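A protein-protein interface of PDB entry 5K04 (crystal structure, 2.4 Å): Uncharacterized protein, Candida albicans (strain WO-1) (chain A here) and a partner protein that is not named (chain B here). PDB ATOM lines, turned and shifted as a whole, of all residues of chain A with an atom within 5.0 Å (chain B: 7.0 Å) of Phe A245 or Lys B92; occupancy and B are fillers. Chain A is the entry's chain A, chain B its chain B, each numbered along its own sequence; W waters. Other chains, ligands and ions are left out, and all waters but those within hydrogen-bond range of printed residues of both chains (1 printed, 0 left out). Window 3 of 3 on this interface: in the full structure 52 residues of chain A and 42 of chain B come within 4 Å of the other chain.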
ATOM      1  N   LEU A 213      21.216   7.641   4.425  1.00  0.00           N
ATOM      2  CA  LEU A 213      22.627   7.279   4.568  1.00  0.00           C
ATOM      3  C   LEU A 213      22.809   6.217   5.648  1.00  0.00           C
ATOM      4  O   LEU A 213      23.559   5.259   5.464  1.00  0.00           O
ATOM      5  CB  LEU A 213      23.469   8.525   4.888  1.00  0.00           C
ATOM      6  CG  LEU A 213      24.984   8.262   4.893  1.00  0.00           C
ATOM      7  CD1 LEU A 213      25.435   7.598   3.575  1.00  0.00           C
ATOM      8  CD2 LEU A 213      25.780   9.528   5.140  1.00  0.00           C
ATOM      9  N   LEU A 239      26.406   3.590  -6.396  1.00  0.00           N
ATOM     10  CA  LEU A 239      26.615   4.798  -5.604  1.00  0.00           C
ATOM     11  C   LEU A 239      27.741   5.639  -6.174  1.00  0.00           C
ATOM     12  O   LEU A 239      27.618   6.863  -6.273  1.00  0.00           O
ATOM     13  CB  LEU A 239      26.929   4.443  -4.151  1.00  0.00           C
ATOM     14  CG  LEU A 239      25.859   3.736  -3.337  1.00  0.00           C
ATOM     15  CD1 LEU A 239      26.328   3.561  -1.894  1.00  0.00           C
ATOM     16  CD2 LEU A 239      24.558   4.503  -3.419  1.00  0.00           C
ATOM     17  N   LEU A 240      28.838   4.988  -6.576  1.00  0.00           N
ATOM     18  CA  LEU A 240      30.067   5.694  -6.926  1.00  0.00           C
ATOM     19  C   LEU A 240      30.025   6.266  -8.341  1.00  0.00           C
ATOM     20  O   LEU A 240      30.446   7.409  -8.563  1.00  0.00           O
ATOM     21  CB  LEU A 240      31.261   4.749  -6.783  1.00  0.00           C
ATOM     22  CG  LEU A 240      31.477   4.171  -5.378  1.00  0.00           C
ATOM     23  CD1 LEU A 240      32.433   2.977  -5.434  1.00  0.00           C
ATOM     24  CD2 LEU A 240      31.972   5.239  -4.404  1.00  0.00           C
ATOM     25  N   GLU A 243      25.640   7.931  -8.775  1.00  0.00           N
ATOM     26  CA  GLU A 243      24.975   8.783  -7.792  1.00  0.00           C
ATOM     27  C   GLU A 243      25.944   9.754  -7.118  1.00  0.00           C
ATOM     28  O   GLU A 243      25.624  10.321  -6.063  1.00  0.00           O
ATOM     29  CB  GLU A 243      24.244   7.912  -6.766  1.00  0.00           C
ATOM     30  CG  GLU A 243      23.110   7.095  -7.433  1.00  0.00           C
ATOM     31  CD  GLU A 243      22.296   6.242  -6.461  1.00  0.00           C
ATOM     32  OE1 GLU A 243      21.442   5.472  -6.945  1.00  0.00           O
ATOM     33  OE2 GLU A 243      22.503   6.333  -5.230  1.00  0.00           O
ATOM     34  N   LYS A 244      27.111   9.960  -7.731  1.00  0.00           N
ATOM     35  CA  LYS A 244      28.160  10.903  -7.311  1.00  0.00           C
ATOM     36  C   LYS A 244      28.285  10.985  -5.791  1.00  0.00           C
ATOM     37  O   LYS A 244      28.226  12.053  -5.173  1.00  0.00           O
ATOM     38  CB  LYS A 244      27.940  12.306  -7.908  1.00  0.00           C
ATOM     39  CG  LYS A 244      26.522  12.848  -7.963  1.00  0.00           C
ATOM     40  CD  LYS A 244      26.402  13.754  -9.179  1.00  0.00           C
ATOM     41  CE  LYS A 244      25.060  14.455  -9.246  1.00  0.00           C
ATOM     42  NZ  LYS A 244      25.004  15.393 -10.408  1.00  0.00           N
ATOM     43  N   PHE A 245      28.490   9.818  -5.198  1.00  0.00           N
ATOM     44  CA  PHE A 245      28.703   9.753  -3.766  1.00  0.00           C
ATOM     45  C   PHE A 245      30.156  10.085  -3.412  1.00  0.00           C
ATOM     46  O   PHE A 245      30.408  10.970  -2.586  1.00  0.00           O
ATOM     47  CB  PHE A 245      28.271   8.380  -3.251  1.00  0.00           C
ATOM     48  CG  PHE A 245      28.176   8.309  -1.767  1.00  0.00           C
ATOM     49  CD1 PHE A 245      28.038   9.465  -1.019  1.00  0.00           C
ATOM     50  CD2 PHE A 245      28.272   7.090  -1.112  1.00  0.00           C
ATOM     51  CE1 PHE A 245      27.978   9.414   0.354  1.00  0.00           C
ATOM     52  CE2 PHE A 245      28.209   7.026   0.255  1.00  0.00           C
ATOM     53  CZ  PHE A 245      28.067   8.197   0.994  1.00  0.00           C
ATOM     54  N   ASP A 246      31.120   9.434  -4.066  1.00  0.00           N
ATOM     55  CA  ASP A 246      32.564   9.713  -3.894  1.00  0.00           C
ATOM     56  C   ASP A 246      32.989   9.556  -2.435  1.00  0.00           C
ATOM     57  O   ASP A 246      33.421  10.501  -1.772  1.00  0.00           O
ATOM     58  CB  ASP A 246      32.963  11.093  -4.414  1.00  0.00           C
ATOM     59  CG  ASP A 246      34.491  11.316  -4.370  1.00  0.00           C
ATOM     60  OD1 ASP A 246      35.249  10.335  -4.227  1.00  0.00           O
ATOM     61  OD2 ASP A 246      34.937  12.479  -4.466  1.00  0.00           O
ATOM     62  N   ASP A 247      32.878   8.317  -1.961  1.00  0.00           N
ATOM     63  CA  ASP A 247      32.982   7.967  -0.549  1.00  0.00           C
ATOM     64  C   ASP A 247      34.062   6.903  -0.383  1.00  0.00           C
ATOM     65  O   ASP A 247      33.940   5.800  -0.931  1.00  0.00           O
ATOM     66  CB  ASP A 247      31.624   7.468  -0.058  1.00  0.00           C
ATOM     67  CG  ASP A 247      31.567   7.301   1.420  1.00  0.00           C
ATOM     68  OD1 ASP A 247      31.571   8.326   2.137  1.00  0.00           O
ATOM     69  OD2 ASP A 247      31.470   6.134   1.854  1.00  0.00           O
ATOM     70  N   THR A 250      33.145   3.493   0.739  1.00  0.00           N
ATOM     71  CA  THR A 250      32.395   2.815  -0.311  1.00  0.00           C
ATOM     72  C   THR A 250      33.303   2.380  -1.461  1.00  0.00           C
ATOM     73  O   THR A 250      33.048   1.343  -2.091  1.00  0.00           O
ATOM     74  CB  THR A 250      31.270   3.727  -0.818  1.00  0.00           C
ATOM     75  OG1 THR A 250      30.486   4.181   0.298  1.00  0.00           O
ATOM     76  CG2 THR A 250      30.364   2.972  -1.806  1.00  0.00           C
ATOM     77  N   THR B   2      37.983  11.113   2.055  1.00  0.00           N
ATOM     78  CA  THR B   2      36.863  11.390   2.947  1.00  0.00           C
ATOM     79  C   THR B   2      35.747  10.376   2.733  1.00  0.00           C
ATOM     80  O   THR B   2      35.527   9.873   1.621  1.00  0.00           O
ATOM     81  CB  THR B   2      36.302  12.835   2.758  1.00  0.00           C
ATOM     82  OG1 THR B   2      35.198  12.842   1.853  1.00  0.00           O
ATOM     83  CG2 THR B   2      37.402  13.772   2.248  1.00  0.00           C
ATOM     84  N   SER B   3      35.088  10.035   3.827  1.00  0.00           N
ATOM     85  CA  SER B   3      33.820   9.334   3.789  1.00  0.00           C
ATOM     86  C   SER B   3      32.806  10.169   4.560  1.00  0.00           C
ATOM     87  O   SER B   3      33.166  10.986   5.413  1.00  0.00           O
ATOM     88  CB  SER B   3      33.934   7.913   4.371  1.00  0.00           C
ATOM     89  OG  SER B   3      35.033   7.218   3.787  1.00  0.00           O
ATOM     90  N   ILE B   4      31.531   9.988   4.243  1.00  0.00           N
ATOM     91  CA  ILE B   4      30.471  10.773   4.853  1.00  0.00           C
ATOM     92  C   ILE B   4      29.629   9.861   5.729  1.00  0.00           C
ATOM     93  O   ILE B   4      29.246   8.757   5.313  1.00  0.00           O
ATOM     94  CB  ILE B   4      29.635  11.494   3.782  1.00  0.00           C
ATOM     95  CG1 ILE B   4      30.465  12.655   3.219  1.00  0.00           C
ATOM     96  CG2 ILE B   4      28.357  12.036   4.373  1.00  0.00           C
ATOM     97  CD1 ILE B   4      29.832  13.367   2.047  1.00  0.00           C
ATOM     98  N   LYS B   5      29.358  10.322   6.951  1.00  0.00           N
ATOM     99  CA  LYS B   5      28.606   9.593   7.958  1.00  0.00           C
ATOM    100  C   LYS B   5      27.555  10.496   8.596  1.00  0.00           C
ATOM    101  O   LYS B   5      27.719  11.721   8.664  1.00  0.00           O
ATOM    102  CB  LYS B   5      29.501   9.023   9.070  1.00  0.00           C
ATOM    103  CG  LYS B   5      30.719   8.215   8.626  1.00  0.00           C
ATOM    104  CD  LYS B   5      30.376   6.940   7.873  1.00  0.00           C
ATOM    105  CE  LYS B   5      31.666   6.315   7.336  1.00  0.00           C
ATOM    106  NZ  LYS B   5      31.444   5.170   6.378  1.00  0.00           N
ATOM    107  N   TYR B  44      25.346  15.845   8.553  1.00  0.00           N
ATOM    108  CA  TYR B  44      26.289  14.769   8.318  1.00  0.00           C
ATOM    109  C   TYR B  44      27.702  15.323   8.400  1.00  0.00           C
ATOM    110  O   TYR B  44      27.942  16.531   8.294  1.00  0.00           O
ATOM    111  CB  TYR B  44      26.064  14.085   6.958  1.00  0.00           C
ATOM    112  CG  TYR B  44      25.911  15.051   5.811  1.00  0.00           C
ATOM    113  CD1 TYR B  44      27.018  15.504   5.097  1.00  0.00           C
ATOM    114  CD2 TYR B  44      24.662  15.509   5.433  1.00  0.00           C
ATOM    115  CE1 TYR B  44      26.869  16.396   4.016  1.00  0.00           C
ATOM    116  CE2 TYR B  44      24.501  16.406   4.365  1.00  0.00           C
ATOM    117  CZ  TYR B  44      25.603  16.844   3.668  1.00  0.00           C
ATOM    118  OH  TYR B  44      25.434  17.738   2.637  1.00  0.00           O
ATOM    119  N   SER B  46      32.034  14.638   7.546  1.00  0.00           N
ATOM    120  CA  SER B  46      33.097  13.997   6.801  1.00  0.00           C
ATOM    121  C   SER B  46      34.057  13.369   7.793  1.00  0.00           C
ATOM    122  O   SER B  46      34.210  13.844   8.922  1.00  0.00           O
ATOM    123  CB  SER B  46      33.830  14.991   5.893  1.00  0.00           C
ATOM    124  OG  SER B  46      34.371  16.089   6.625  1.00  0.00           O
ATOM    125  N   ILE B  87      41.172  20.972  -0.556  1.00  0.00           N
ATOM    126  CA  ILE B  87      41.081  19.753  -1.357  1.00  0.00           C
ATOM    127  C   ILE B  87      39.622  19.480  -1.715  1.00  0.00           C
ATOM    128  O   ILE B  87      39.267  18.350  -2.069  1.00  0.00           O
ATOM    129  CB  ILE B  87      41.701  18.540  -0.630  1.00  0.00           C
ATOM    130  CG1 ILE B  87      41.020  18.327   0.729  1.00  0.00           C
ATOM    131  CG2 ILE B  87      43.226  18.721  -0.460  1.00  0.00           C
ATOM    132  CD1 ILE B  87      41.497  17.089   1.462  1.00  0.00           C
ATOM    133  N   GLY B  88      38.771  20.508  -1.622  1.00  0.00           N
ATOM    134  CA  GLY B  88      37.387  20.394  -2.067  1.00  0.00           C
ATOM    135  C   GLY B  88      36.434  19.729  -1.096  1.00  0.00           C
ATOM    136  O   GLY B  88      35.333  19.334  -1.492  1.00  0.00           O
ATOM    137  N   LEU B  89      36.824  19.586   0.168  1.00  0.00           N
ATOM    138  CA  LEU B  89      35.962  18.908   1.126  1.00  0.00           C
ATOM    139  C   LEU B  89      34.715  19.738   1.435  1.00  0.00           C
ATOM    140  O   LEU B  89      33.597  19.201   1.478  1.00  0.00           O
ATOM    141  CB  LEU B  89      36.767  18.600   2.389  1.00  0.00           C
ATOM    142  CG  LEU B  89      36.048  17.887   3.520  1.00  0.00           C
ATOM    143  CD1 LEU B  89      35.276  16.691   2.992  1.00  0.00           C
ATOM    144  CD2 LEU B  89      37.089  17.453   4.558  1.00  0.00           C
ATOM    145  N   ALA B  90      34.886  21.047   1.651  1.00  0.00           N
ATOM    146  CA  ALA B  90      33.732  21.919   1.845  1.00  0.00           C
ATOM    147  C   ALA B  90      32.811  21.880   0.630  1.00  0.00           C
ATOM    148  O   ALA B  90      31.585  21.763   0.766  1.00  0.00           O
ATOM    149  CB  ALA B  90      34.199  23.350   2.122  1.00  0.00           C
ATOM    150  N   SER B  91      33.392  21.960  -0.570  1.00  0.00           N
ATOM    151  CA  SER B  91      32.587  21.869  -1.782  1.00  0.00           C
ATOM    152  C   SER B  91      31.846  20.530  -1.862  1.00  0.00           C
ATOM    153  O   SER B  91      30.695  20.478  -2.314  1.00  0.00           O
ATOM    154  CB  SER B  91      33.483  22.093  -3.001  1.00  0.00           C
ATOM    155  OG  SER B  91      34.125  23.351  -2.928  1.00  0.00           O
ATOM    156  N   LYS B  92      32.478  19.442  -1.403  1.00  0.00           N
ATOM    157  CA  LYS B  92      31.826  18.133  -1.437  1.00  0.00           C
ATOM    158  C   LYS B  92      30.649  18.066  -0.467  1.00  0.00           C
ATOM    159  O   LYS B  92      29.582  17.548  -0.814  1.00  0.00           O
ATOM    160  CB  LYS B  92      32.835  17.021  -1.127  1.00  0.00           C
ATOM    161  CG  LYS B  92      32.226  15.808  -0.394  1.00  0.00           C
ATOM    162  CD  LYS B  92      33.199  14.629  -0.225  1.00  0.00           C
ATOM    163  CE  LYS B  92      32.952  13.558  -1.282  1.00  0.00           C
ATOM    164  NZ  LYS B  92      31.581  12.928  -1.164  1.00  0.00           N
ATOM    165  N   LEU B  93      30.834  18.581   0.753  1.00  0.00           N
ATOM    166  CA  LEU B  93      29.758  18.614   1.745  1.00  0.00           C
ATOM    167  C   LEU B  93      28.547  19.399   1.240  1.00  0.00           C
ATOM    168  O   LEU B  93      27.396  18.987   1.450  1.00  0.00           O
ATOM    169  CB  LEU B  93      30.280  19.224   3.047  1.00  0.00           C
ATOM    170  CG  LEU B  93      31.259  18.358   3.846  1.00  0.00           C
ATOM    171  CD1 LEU B  93      31.977  19.194   4.886  1.00  0.00           C
ATOM    172  CD2 LEU B  93      30.532  17.198   4.514  1.00  0.00           C
ATOM    173  N   CYS B  94      28.790  20.533   0.569  1.00  0.00           N
ATOM    174  CA  CYS B  94      27.696  21.318   0.006  1.00  0.00           C
ATOM    175  C   CYS B  94      27.034  20.586  -1.169  1.00  0.00           C
ATOM    176  O   CYS B  94      25.801  20.568  -1.286  1.00  0.00           O
ATOM    177  CB  CYS B  94      28.213  22.714  -0.404  1.00  0.00           C
ATOM    178  SG  CYS B  94      28.842  23.758   0.893  1.00  0.00           S
ATOM    179  N   LEU B  95      27.837  19.930  -2.017  1.00  0.00           N
ATOM    180  CA  LEU B  95      27.300  19.228  -3.182  1.00  0.00           C
ATOM    181  C   LEU B  95      26.526  17.956  -2.807  1.00  0.00           C
ATOM    182  O   LEU B  95      25.586  17.577  -3.510  1.00  0.00           O
ATOM    183  CB  LEU B  95      28.438  18.897  -4.135  1.00  0.00           C
ATOM    184  CG  LEU B  95      28.965  20.043  -4.991  1.00  0.00           C
ATOM    185  CD1 LEU B  95      30.030  19.513  -5.954  1.00  0.00           C
ATOM    186  CD2 LEU B  95      27.826  20.711  -5.758  1.00  0.00           C
ATOM    187  N   GLU B  96      26.897  17.299  -1.706  1.00  0.00           N
ATOM    188  CA  GLU B  96      26.187  16.105  -1.243  1.00  0.00           C
ATOM    189  C   GLU B  96      24.717  16.389  -0.908  1.00  0.00           C
ATOM    190  O   GLU B  96      23.879  15.483  -0.983  1.00  0.00           O
ATOM    191  CB  GLU B  96      26.916  15.530  -0.021  1.00  0.00           C
ATOM    192  CG  GLU B  96      26.144  14.484   0.801  1.00  0.00           C
ATOM    193  CD  GLU B  96      25.904  13.158   0.080  1.00  0.00           C
ATOM    194  OE1 GLU B  96      25.134  12.330   0.622  1.00  0.00           O
ATOM    195  OE2 GLU B  96      26.480  12.930  -1.010  1.00  0.00           O
ATOM    196  N   LEU B  97      24.390  17.627  -0.511  1.00  0.00           N
ATOM    197  CA  LEU B  97      22.994  18.000  -0.286  1.00  0.00           C
ATOM    198  C   LEU B  97      22.139  17.700  -1.512  1.00  0.00           C
ATOM    199  O   LEU B  97      21.013  17.205  -1.392  1.00  0.00           O
ATOM    200  CB  LEU B  97      22.901  19.483   0.065  1.00  0.00           C
ATOM    201  CG  LEU B  97      23.407  19.878   1.447  1.00  0.00           C
ATOM    202  CD1 LEU B  97      23.525  21.388   1.561  1.00  0.00           C
ATOM    203  CD2 LEU B  97      22.464  19.350   2.494  1.00  0.00           C
ATOM    204  N   ASN B  99      22.280  15.423  -3.571  1.00  0.00           N
ATOM    205  CA  ASN B  99      22.011  13.990  -3.688  1.00  0.00           C
ATOM    206  C   ASN B  99      20.869  13.502  -2.804  1.00  0.00           C
ATOM    207  O   ASN B  99      20.330  12.416  -3.054  1.00  0.00           O
ATOM    208  CB  ASN B  99      23.263  13.187  -3.326  1.00  0.00           C
ATOM    209  CG  ASN B  99      24.389  13.381  -4.327  1.00  0.00           C
ATOM    210  OD1 ASN B  99      24.164  13.830  -5.462  1.00  0.00           O
ATOM    211  ND2 ASN B  99      25.609  13.027  -3.918  1.00  0.00           N
ATOM    212  N   LEU B 127      30.320  26.698  -6.918  1.00  0.00           N
ATOM    213  CA  LEU B 127      29.361  25.605  -6.799  1.00  0.00           C
ATOM    214  C   LEU B 127      28.057  25.859  -7.548  1.00  0.00           C
ATOM    215  O   LEU B 127      27.167  25.006  -7.508  1.00  0.00           O
ATOM    216  CB  LEU B 127      29.047  25.350  -5.329  1.00  0.00           C
ATOM    217  CG  LEU B 127      30.225  24.833  -4.502  1.00  0.00           C
ATOM    218  CD1 LEU B 127      29.799  24.575  -3.061  1.00  0.00           C
ATOM    219  CD2 LEU B 127      30.807  23.567  -5.129  1.00  0.00           C
HETATM  220  O   HOH W   1      30.589   6.251   4.367  1.00  0.00           O
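Water W1 lies within hydrogen-bond range of NZ of Lys B5 (2.4 Å), OD2 of Asp A247 (2.7 Å) and O of Ile B4 (3.0 Å).
Of the printed residues of chain B, Glu A243 touches Asn B99. Phe A245 touches just these residues of chain B: Lys B92 and Glu B96. Printed residues of chain A within 4 Å of Ser B3: Asp A247 (3.0 Å). Of the printed residues of chain A, Ile B4 touches Leu A213 (3.6 Å) and Asp A247 (2.7 Å). Lys B92 touches just these residues of chain A: Phe A245 (2.7 Å) and Asp A246 (3.1 Å). Printed residues of chain A within 4 Å of Asn B99: Glu A243 (3.5 Å) and Lys A244 (3.1 Å). The nearest residue of chain B that does not touch Phe A245 is Ile B4 (4.3 Å). The nearest residue of chain A that does not touch Lys B92 is Asp A247 (4.9 Å).
Among the printed residues, pairs that only touch across the chains: Asp A247 with Ser B3 (3.0 Å), Leu A213 with Ile B4 (3.6 Å), Phe A245 with Glu B96 (3.8 Å), Asp A247 with Thr B2 (3.8 Å) and Leu A213 with Lys B5 (3.99 Å).
Of the 9 printed residues of chain A, 6 touch a printed residue of chain B. Along chain A the printed residues that touch a printed residue of chain B span positions 213 to 247. Of the 19 printed residues of chain B, 7 touch a printed residue of chain A. Printed residues of chain B that touch a printed residue of chain A: Thr B2, Ser B3, Ile B4, Lys B5, Lys B92, Glu B96 and Asn B99. Among the printed residues, no Asp or Glu carboxylate lies within 4 Å of a Lys or Arg side-chain nitrogen of the other chain.
The backbone carbonyl oxygen (O) of Leu A239 is in hydrogen-bond range of the backbone NH (N) of Lys A244, 3.5 Å away. The backbone NH (N) of Phe A245 sits at hydrogen-bond distance from the backbone carbonyl oxygen (O) of Leu A239 (3.3 Å). The side-chain carboxylate (OD2) of Asp A247 is in hydrogen-bond range of the side-chain hydroxyl (OG1) of Thr A250 (2.7 Å). OE2 of Glu B96 sits at hydrogen-bond distance from ND2 of Asn B99 (3.0 Å).
ND2 of Asn B99 sits at hydrogen-bond distance from O of Glu A243, 3.5 Å away. The side-chain amide nitrogen (ND2) of Asn B99 lies within hydrogen-bond range of the backbone carbonyl oxygen (O) of Lys A244 (3.1 Å). NZ of Lys B92 is in hydrogen-bond range of O of Phe A245, 2.7 Å away. The backbone carbonyl oxygen (O) of Asp A246 sits at hydrogen-bond distance from the side-chain amino group (NZ) of Lys B92 (3.1 Å). The side-chain carboxylate (OD1) of Asp A247 lies within hydrogen-bond range of the backbone NH (N) of Ile B4 (2.7 Å).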
